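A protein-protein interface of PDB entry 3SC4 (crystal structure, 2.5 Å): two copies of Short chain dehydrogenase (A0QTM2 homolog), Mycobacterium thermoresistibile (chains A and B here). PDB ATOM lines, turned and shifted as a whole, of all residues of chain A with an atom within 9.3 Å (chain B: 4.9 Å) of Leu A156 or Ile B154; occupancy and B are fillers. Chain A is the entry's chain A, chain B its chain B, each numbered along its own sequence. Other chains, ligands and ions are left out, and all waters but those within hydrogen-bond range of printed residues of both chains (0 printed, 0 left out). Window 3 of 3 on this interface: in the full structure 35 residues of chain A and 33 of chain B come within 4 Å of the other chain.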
ATOM      1  N   PRO A 153       0.237  28.499  18.539  1.00  0.00           N
ATOM      2  CA  PRO A 153       1.032  27.273  18.590  1.00  0.00           C
ATOM      3  C   PRO A 153       2.271  27.524  19.426  1.00  0.00           C
ATOM      4  O   PRO A 153       2.744  28.667  19.465  1.00  0.00           O
ATOM      5  CB  PRO A 153       1.473  27.040  17.132  1.00  0.00           C
ATOM      6  CG  PRO A 153       0.737  27.979  16.320  1.00  0.00           C
ATOM      7  CD  PRO A 153       0.263  29.109  17.208  1.00  0.00           C
ATOM      8  N   ILE A 154       2.758  26.475  20.087  1.00  0.00           N
ATOM      9  CA  ILE A 154       3.963  26.541  20.894  1.00  0.00           C
ATOM     10  C   ILE A 154       5.157  26.368  19.974  1.00  0.00           C
ATOM     11  O   ILE A 154       5.341  25.314  19.404  1.00  0.00           O
ATOM     12  CB  ILE A 154       4.041  25.427  21.941  1.00  0.00           C
ATOM     13  CG1 ILE A 154       2.810  25.429  22.858  1.00  0.00           C
ATOM     14  CG2 ILE A 154       5.380  25.544  22.762  1.00  0.00           C
ATOM     15  CD1 ILE A 154       2.639  26.689  23.660  1.00  0.00           C
ATOM     16  N   ARG A 155       5.964  27.410  19.847  1.00  0.00           N
ATOM     17  CA  ARG A 155       7.148  27.359  19.037  1.00  0.00           C
ATOM     18  C   ARG A 155       8.387  27.574  19.901  1.00  0.00           C
ATOM     19  O   ARG A 155       8.511  28.592  20.583  1.00  0.00           O
ATOM     20  CB  ARG A 155       7.017  28.419  17.952  1.00  0.00           C
ATOM     21  CG  ARG A 155       5.650  28.342  17.276  1.00  0.00           C
ATOM     22  CD  ARG A 155       5.661  28.818  15.884  1.00  0.00           C
ATOM     23  NE  ARG A 155       6.692  28.216  15.054  1.00  0.00           N
ATOM     24  CZ  ARG A 155       6.920  28.610  13.805  1.00  0.00           C
ATOM     25  NH1 ARG A 155       6.195  29.588  13.277  1.00  0.00           N
ATOM     26  NH2 ARG A 155       7.870  28.037  13.086  1.00  0.00           N
ATOM     27  N   LEU A 156       9.311  26.621  19.828  1.00  0.00           N
ATOM     28  CA  LEU A 156      10.426  26.525  20.777  1.00  0.00           C
ATOM     29  C   LEU A 156      11.749  27.043  20.259  1.00  0.00           C
ATOM     30  O   LEU A 156      12.707  27.101  21.014  1.00  0.00           O
ATOM     31  CB  LEU A 156      10.610  25.068  21.220  1.00  0.00           C
ATOM     32  CG  LEU A 156       9.415  24.538  22.028  1.00  0.00           C
ATOM     33  CD1 LEU A 156       9.685  23.110  22.507  1.00  0.00           C
ATOM     34  CD2 LEU A 156       9.090  25.491  23.179  1.00  0.00           C
ATOM     35  N   GLU A 157      11.807  27.388  18.979  1.00  0.00           N
ATOM     36  CA  GLU A 157      12.991  28.014  18.408  1.00  0.00           C
ATOM     37  C   GLU A 157      13.249  29.349  19.148  1.00  0.00           C
ATOM     38  O   GLU A 157      12.338  30.130  19.377  1.00  0.00           O
ATOM     39  CB  GLU A 157      12.829  28.258  16.873  1.00  0.00           C
ATOM     40  CG  GLU A 157      12.635  26.962  15.955  1.00  0.00           C
ATOM     41  CD  GLU A 157      11.196  26.361  15.961  1.00  0.00           C
ATOM     42  OE1 GLU A 157      10.241  27.015  16.424  1.00  0.00           O
ATOM     43  OE2 GLU A 157      11.018  25.207  15.517  1.00  0.00           O
ATOM     44  N   PRO A 158      14.501  29.604  19.531  1.00  0.00           N
ATOM     45  CA  PRO A 158      14.932  30.796  20.252  1.00  0.00           C
ATOM     46  C   PRO A 158      14.231  32.090  19.881  1.00  0.00           C
ATOM     47  O   PRO A 158      13.863  32.864  20.757  1.00  0.00           O
ATOM     48  CB  PRO A 158      16.416  30.893  19.875  1.00  0.00           C
ATOM     49  CG  PRO A 158      16.851  29.499  19.785  1.00  0.00           C
ATOM     50  CD  PRO A 158      15.649  28.724  19.241  1.00  0.00           C
ATOM     51  N   LYS A 159      14.046  32.339  18.597  1.00  0.00           N
ATOM     52  CA  LYS A 159      13.494  33.617  18.177  1.00  0.00           C
ATOM     53  C   LYS A 159      12.043  33.834  18.589  1.00  0.00           C
ATOM     54  O   LYS A 159      11.570  34.968  18.584  1.00  0.00           O
ATOM     55  CB  LYS A 159      13.634  33.776  16.670  1.00  0.00           C
ATOM     56  CG  LYS A 159      12.912  32.697  15.845  1.00  0.00           C
ATOM     57  CD  LYS A 159      12.425  33.258  14.511  1.00  0.00           C
ATOM     58  CE  LYS A 159      12.325  32.169  13.442  1.00  0.00           C
ATOM     59  NZ  LYS A 159      11.996  32.794  12.111  1.00  0.00           N
ATOM     60  N   TRP A 160      11.332  32.758  18.946  1.00  0.00           N
ATOM     61  CA  TRP A 160       9.940  32.855  19.360  1.00  0.00           C
ATOM     62  C   TRP A 160       9.764  32.992  20.863  1.00  0.00           C
ATOM     63  O   TRP A 160       8.639  33.226  21.344  1.00  0.00           O
ATOM     64  CB  TRP A 160       9.183  31.608  18.945  1.00  0.00           C
ATOM     65  CG  TRP A 160       9.194  31.315  17.489  1.00  0.00           C
ATOM     66  CD1 TRP A 160       9.599  30.169  16.896  1.00  0.00           C
ATOM     67  CD2 TRP A 160       8.733  32.172  16.449  1.00  0.00           C
ATOM     68  NE1 TRP A 160       9.453  30.263  15.545  1.00  0.00           N
ATOM     69  CE2 TRP A 160       8.928  31.490  15.240  1.00  0.00           C
ATOM     70  CE3 TRP A 160       8.176  33.454  16.423  1.00  0.00           C
ATOM     71  CZ2 TRP A 160       8.589  32.047  14.001  1.00  0.00           C
ATOM     72  CZ3 TRP A 160       7.845  34.023  15.180  1.00  0.00           C
ATOM     73  CH2 TRP A 160       8.048  33.321  13.999  1.00  0.00           C
ATOM     74  N   LEU A 161      10.855  32.812  21.610  1.00  0.00           N
ATOM     75  CA  LEU A 161      10.776  32.749  23.053  1.00  0.00           C
ATOM     76  C   LEU A 161      10.909  34.133  23.678  1.00  0.00           C
ATOM     77  O   LEU A 161      11.243  34.279  24.838  1.00  0.00           O
ATOM     78  CB  LEU A 161      11.817  31.772  23.593  1.00  0.00           C
ATOM     79  CG  LEU A 161      11.612  30.323  23.128  1.00  0.00           C
ATOM     80  CD1 LEU A 161      12.803  29.459  23.512  1.00  0.00           C
ATOM     81  CD2 LEU A 161      10.322  29.732  23.677  1.00  0.00           C
ATOM     82  N   ARG A 162      10.626  35.168  22.912  1.00  0.00           N
ATOM     83  CA  ARG A 162      10.494  36.473  23.502  1.00  0.00           C
ATOM     84  C   ARG A 162       9.385  37.334  22.887  1.00  0.00           C
ATOM     85  O   ARG A 162       8.880  37.045  21.811  1.00  0.00           O
ATOM     86  CB  ARG A 162      11.854  37.166  23.545  1.00  0.00           C
ATOM     87  CG  ARG A 162      12.594  37.439  22.276  1.00  0.00           C
ATOM     88  CD  ARG A 162      14.079  37.404  22.639  1.00  0.00           C
ATOM     89  NE  ARG A 162      14.976  37.988  21.655  1.00  0.00           N
ATOM     90  CZ  ARG A 162      15.512  39.211  21.729  1.00  0.00           C
ATOM     91  NH1 ARG A 162      15.244  40.061  22.739  1.00  0.00           N
ATOM     92  NH2 ARG A 162      16.328  39.602  20.772  1.00  0.00           N
ATOM     93  N   MET A 167       5.086  35.858  26.165  1.00  0.00           N
ATOM     94  CA  MET A 167       5.222  34.508  25.651  1.00  0.00           C
ATOM     95  C   MET A 167       4.827  33.494  26.734  1.00  0.00           C
ATOM     96  O   MET A 167       4.146  32.533  26.431  1.00  0.00           O
ATOM     97  CB  MET A 167       6.646  34.266  25.158  1.00  0.00           C
ATOM     98  CG  MET A 167       6.943  32.839  24.720  1.00  0.00           C
ATOM     99  SD  MET A 167       7.298  31.730  26.115  1.00  0.00           S
ATOM    100  CE  MET A 167       8.860  32.386  26.671  1.00  0.00           C
ATOM    101  N   TYR A 171       1.655  31.222  25.787  1.00  0.00           N
ATOM    102  CA  TYR A 171       2.009  29.797  25.747  1.00  0.00           C
ATOM    103  C   TYR A 171       1.337  29.052  26.915  1.00  0.00           C
ATOM    104  O   TYR A 171       0.852  27.946  26.757  1.00  0.00           O
ATOM    105  CB  TYR A 171       3.522  29.587  25.809  1.00  0.00           C
ATOM    106  CG  TYR A 171       4.321  29.768  24.503  1.00  0.00           C
ATOM    107  CD1 TYR A 171       3.842  30.535  23.439  1.00  0.00           C
ATOM    108  CD2 TYR A 171       5.589  29.188  24.364  1.00  0.00           C
ATOM    109  CE1 TYR A 171       4.584  30.707  22.270  1.00  0.00           C
ATOM    110  CE2 TYR A 171       6.336  29.340  23.184  1.00  0.00           C
ATOM    111  CZ  TYR A 171       5.821  30.107  22.139  1.00  0.00           C
ATOM    112  OH  TYR A 171       6.564  30.265  20.974  1.00  0.00           O
ATOM    113  N   LEU A 175      -0.933  25.797  26.622  1.00  0.00           N
ATOM    114  CA  LEU A 175      -0.654  24.541  27.317  1.00  0.00           C
ATOM    115  C   LEU A 175      -1.896  24.063  28.088  1.00  0.00           C
ATOM    116  O   LEU A 175      -2.215  22.891  28.073  1.00  0.00           O
ATOM    117  CB  LEU A 175       0.577  24.676  28.220  1.00  0.00           C
ATOM    118  CG  LEU A 175       1.873  24.836  27.387  1.00  0.00           C
ATOM    119  CD1 LEU A 175       3.002  25.287  28.239  1.00  0.00           C
ATOM    120  CD2 LEU A 175       2.239  23.546  26.627  1.00  0.00           C
ATOM    121  N   LEU A 178      -4.327  22.603  25.692  1.00  0.00           N
ATOM    122  CA  LEU A 178      -3.850  21.305  25.214  1.00  0.00           C
ATOM    123  C   LEU A 178      -3.933  20.206  26.277  1.00  0.00           C
ATOM    124  O   LEU A 178      -4.246  19.051  25.969  1.00  0.00           O
ATOM    125  CB  LEU A 178      -2.435  21.442  24.679  1.00  0.00           C
ATOM    126  CG  LEU A 178      -2.253  22.243  23.376  1.00  0.00           C
ATOM    127  CD1 LEU A 178      -0.773  22.225  22.931  1.00  0.00           C
ATOM    128  CD2 LEU A 178      -3.141  21.664  22.314  1.00  0.00           C
ATOM    129  N   TRP A 273       4.542  34.736  16.436  1.00  0.00           N
ATOM    130  CA  TRP A 273       4.542  33.278  16.349  1.00  0.00           C
ATOM    131  C   TRP A 273       4.108  32.683  15.018  1.00  0.00           C
ATOM    132  O   TRP A 273       3.835  31.484  14.949  1.00  0.00           O
ATOM    133  CB  TRP A 273       3.745  32.660  17.507  1.00  0.00           C
ATOM    134  CG  TRP A 273       4.327  33.037  18.816  1.00  0.00           C
ATOM    135  CD1 TRP A 273       5.557  32.699  19.268  1.00  0.00           C
ATOM    136  CD2 TRP A 273       3.744  33.880  19.810  1.00  0.00           C
ATOM    137  NE1 TRP A 273       5.780  33.262  20.491  1.00  0.00           N
ATOM    138  CE2 TRP A 273       4.676  33.980  20.862  1.00  0.00           C
ATOM    139  CE3 TRP A 273       2.507  34.530  19.935  1.00  0.00           C
ATOM    140  CZ2 TRP A 273       4.428  34.710  22.022  1.00  0.00           C
ATOM    141  CZ3 TRP A 273       2.249  35.277  21.110  1.00  0.00           C
ATOM    142  CH2 TRP A 273       3.203  35.344  22.137  1.00  0.00           C
ATOM    143  N   PRO B 152      11.582  20.767  33.382  1.00  0.00           N
ATOM    144  CA  PRO B 152      11.820  19.775  32.352  1.00  0.00           C
ATOM    145  C   PRO B 152      11.839  20.364  30.965  1.00  0.00           C
ATOM    146  O   PRO B 152      11.369  21.486  30.777  1.00  0.00           O
ATOM    147  CB  PRO B 152      10.586  18.893  32.469  1.00  0.00           C
ATOM    148  CG  PRO B 152       9.482  19.859  32.796  1.00  0.00           C
ATOM    149  CD  PRO B 152      10.133  20.997  33.571  1.00  0.00           C
ATOM    150  N   PRO B 153      12.347  19.610  29.990  1.00  0.00           N
ATOM    151  CA  PRO B 153      12.168  19.977  28.579  1.00  0.00           C
ATOM    152  C   PRO B 153      10.703  20.011  28.229  1.00  0.00           C
ATOM    153  O   PRO B 153       9.912  19.262  28.832  1.00  0.00           O
ATOM    154  CB  PRO B 153      12.806  18.815  27.796  1.00  0.00           C
ATOM    155  CG  PRO B 153      13.571  18.043  28.774  1.00  0.00           C
ATOM    156  CD  PRO B 153      12.940  18.278  30.134  1.00  0.00           C
ATOM    157  N   ILE B 154      10.375  20.873  27.269  1.00  0.00           N
ATOM    158  CA  ILE B 154       9.037  21.064  26.783  1.00  0.00           C
ATOM    159  C   ILE B 154       8.808  19.957  25.780  1.00  0.00           C
ATOM    160  O   ILE B 154       9.392  19.952  24.694  1.00  0.00           O
ATOM    161  CB  ILE B 154       8.834  22.400  26.083  1.00  0.00           C
ATOM    162  CG1 ILE B 154       9.312  23.579  26.957  1.00  0.00           C
ATOM    163  CG2 ILE B 154       7.400  22.546  25.652  1.00  0.00           C
ATOM    164  CD1 ILE B 154       8.598  23.779  28.241  1.00  0.00           C
ATOM    165  N   ARG B 155       7.942  19.026  26.167  1.00  0.00           N
ATOM    166  CA  ARG B 155       7.524  17.899  25.338  1.00  0.00           C
ATOM    167  C   ARG B 155       6.045  18.108  24.973  1.00  0.00           C
ATOM    168  O   ARG B 155       5.199  18.253  25.853  1.00  0.00           O
ATOM    169  CB  ARG B 155       7.668  16.617  26.154  1.00  0.00           C
ATOM    170  CG  ARG B 155       9.114  16.288  26.583  1.00  0.00           C
ATOM    171  CD  ARG B 155       9.726  15.426  25.512  1.00  0.00           C
ATOM    172  NE  ARG B 155      10.254  14.224  26.103  1.00  0.00           N
ATOM    173  CZ  ARG B 155      10.367  13.052  25.498  1.00  0.00           C
ATOM    174  NH1 ARG B 155       9.971  12.851  24.255  1.00  0.00           N
ATOM    175  NH2 ARG B 155      10.902  12.060  26.185  1.00  0.00           N
ATOM    176  N   LEU B 156       5.750  18.105  23.678  1.00  0.00           N
ATOM    177  CA  LEU B 156       4.450  18.535  23.164  1.00  0.00           C
ATOM    178  C   LEU B 156       3.576  17.412  22.631  1.00  0.00           C
ATOM    179  O   LEU B 156       2.423  17.660  22.231  1.00  0.00           O
ATOM    180  CB  LEU B 156       4.656  19.551  22.036  1.00  0.00           C
ATOM    181  CG  LEU B 156       5.335  20.860  22.439  1.00  0.00           C
ATOM    182  CD1 LEU B 156       5.578  21.726  21.178  1.00  0.00           C
ATOM    183  CD2 LEU B 156       4.492  21.586  23.487  1.00  0.00           C
ATOM    184  N   TYR B 171       6.255  23.485  32.866  1.00  0.00           N
ATOM    185  CA  TYR B 171       6.613  24.029  31.566  1.00  0.00           C
ATOM    186  C   TYR B 171       6.764  25.562  31.615  1.00  0.00           C
ATOM    187  O   TYR B 171       7.619  26.144  30.935  1.00  0.00           O
ATOM    188  CB  TYR B 171       5.558  23.652  30.516  1.00  0.00           C
ATOM    189  CG  TYR B 171       5.658  22.232  29.935  1.00  0.00           C
ATOM    190  CD1 TYR B 171       6.364  21.226  30.567  1.00  0.00           C
ATOM    191  CD2 TYR B 171       4.990  21.910  28.778  1.00  0.00           C
ATOM    192  CE1 TYR B 171       6.412  19.926  30.024  1.00  0.00           C
ATOM    193  CE2 TYR B 171       5.036  20.652  28.244  1.00  0.00           C
ATOM    194  CZ  TYR B 171       5.743  19.654  28.867  1.00  0.00           C
ATOM    195  OH  TYR B 171       5.776  18.395  28.301  1.00  0.00           O
ATOM    196  N   THR B 174      10.197  26.354  32.786  1.00  0.00           N
ATOM    197  CA  THR B 174      11.135  26.152  31.679  1.00  0.00           C
ATOM    198  C   THR B 174      11.024  27.293  30.664  1.00  0.00           C
ATOM    199  O   THR B 174      12.017  27.898  30.270  1.00  0.00           O
ATOM    200  CB  THR B 174      10.901  24.765  31.049  1.00  0.00           C
ATOM    201  OG1 THR B 174      11.305  23.736  31.997  1.00  0.00           O
ATOM    202  CG2 THR B 174      11.657  24.612  29.702  1.00  0.00           C
ATOM    203  N   LEU B 175       9.816  27.665  30.284  1.00  0.00           N
ATOM    204  CA  LEU B 175       9.655  28.779  29.330  1.00  0.00           C
ATOM    205  C   LEU B 175      10.255  30.091  29.851  1.00  0.00           C
ATOM    206  O   LEU B 175      10.851  30.874  29.094  1.00  0.00           O
ATOM    207  CB  LEU B 175       8.185  28.963  28.970  1.00  0.00           C
ATOM    208  CG  LEU B 175       7.601  27.877  28.069  1.00  0.00           C
ATOM    209  CD1 LEU B 175       6.104  28.081  27.918  1.00  0.00           C
ATOM    210  CD2 LEU B 175       8.306  27.906  26.702  1.00  0.00           C
ATOM    211  N   LEU B 178      14.041  29.704  29.362  1.00  0.00           N
ATOM    212  CA  LEU B 178      14.433  29.815  27.962  1.00  0.00           C
ATOM    213  C   LEU B 178      14.240  31.222  27.413  1.00  0.00           C
ATOM    214  O   LEU B 178      14.997  31.682  26.575  1.00  0.00           O
ATOM    215  CB  LEU B 178      13.652  28.821  27.099  1.00  0.00           C
ATOM    216  CG  LEU B 178      13.853  27.348  27.457  1.00  0.00           C
ATOM    217  CD1 LEU B 178      13.042  26.439  26.527  1.00  0.00           C
ATOM    218  CD2 LEU B 178      15.344  26.973  27.381  1.00  0.00           C
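O of Arg A155 is in hydrogen-bond range of OH of Tyr A171 (2.6 Å). The side-chain hydroxyl of Tyr A171 lies within hydrogen-bond range of the indole nitrogen of Trp A273, at 3.1 Å. O of Arg B155 lies within hydrogen-bond range of OH of Tyr B171, at 2.5 Å.
CB of Ile B154 touches CD1 of Leu A156, 3.7 Å away. CB of Leu B178 touches CD1 of Leu A161, 3.7 Å away. Met A167 touches Leu B175 (CE to O, 3.5 Å). Tyr A171 touches Leu B175. Leu A175 touches Tyr B171 (CD1 to CB, 3.8 Å).
Of the 9 printed residues of chain B, 4 touch a printed residue of chain A. Printed residues of chain B that touch a printed residue of chain A: Ile B154, Tyr B171, Leu B175 and Leu B178. Hydrophobic or aromatic side chains of chain B within 4 Å of the printed part of chain A: Ile B154, Tyr B171, Leu B175 and Leu B178. Among the printed residues, no Asp or Glu carboxylate lies within 4 Å of a Lys or Arg side-chain nitrogen of the other chain.
Leu A156 touches Ile B154, but with the chains exchanged Ile A154 does not touch Leu B156 (4.01 Å). Tyr A171 touches Leu B175, and with the chains exchanged Leu A175 touches Tyr B171.
Of chain B, only Ile B154 (3.7 Å) comes within 4 Å of Leu A156. Of chain A, only Leu A156 comes within 4 Å of Ile B154. No residue of chain A comes within 4 Å of Pro B153. Of the printed residues of chain B, Leu A175 touches Tyr B171. Printed residues of chain B within 4 Å of Leu A161: Leu B178 (3.7 Å). Of the printed residues of chain A, Leu B175 touches Met A167 and Tyr A171. Printed residues of chain B within 4 Å of Tyr A171: Leu B175. Printed residues of chain A within 4 Å of Leu B178: Leu A161 (3.7 Å). Pro A158 touches none of the printed residues of chain B. Trp A160 touches none of the printed residues of chain B. The nearest residue of chain A that does not touch Ile B154 is Ile A154 (4.6 Å).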
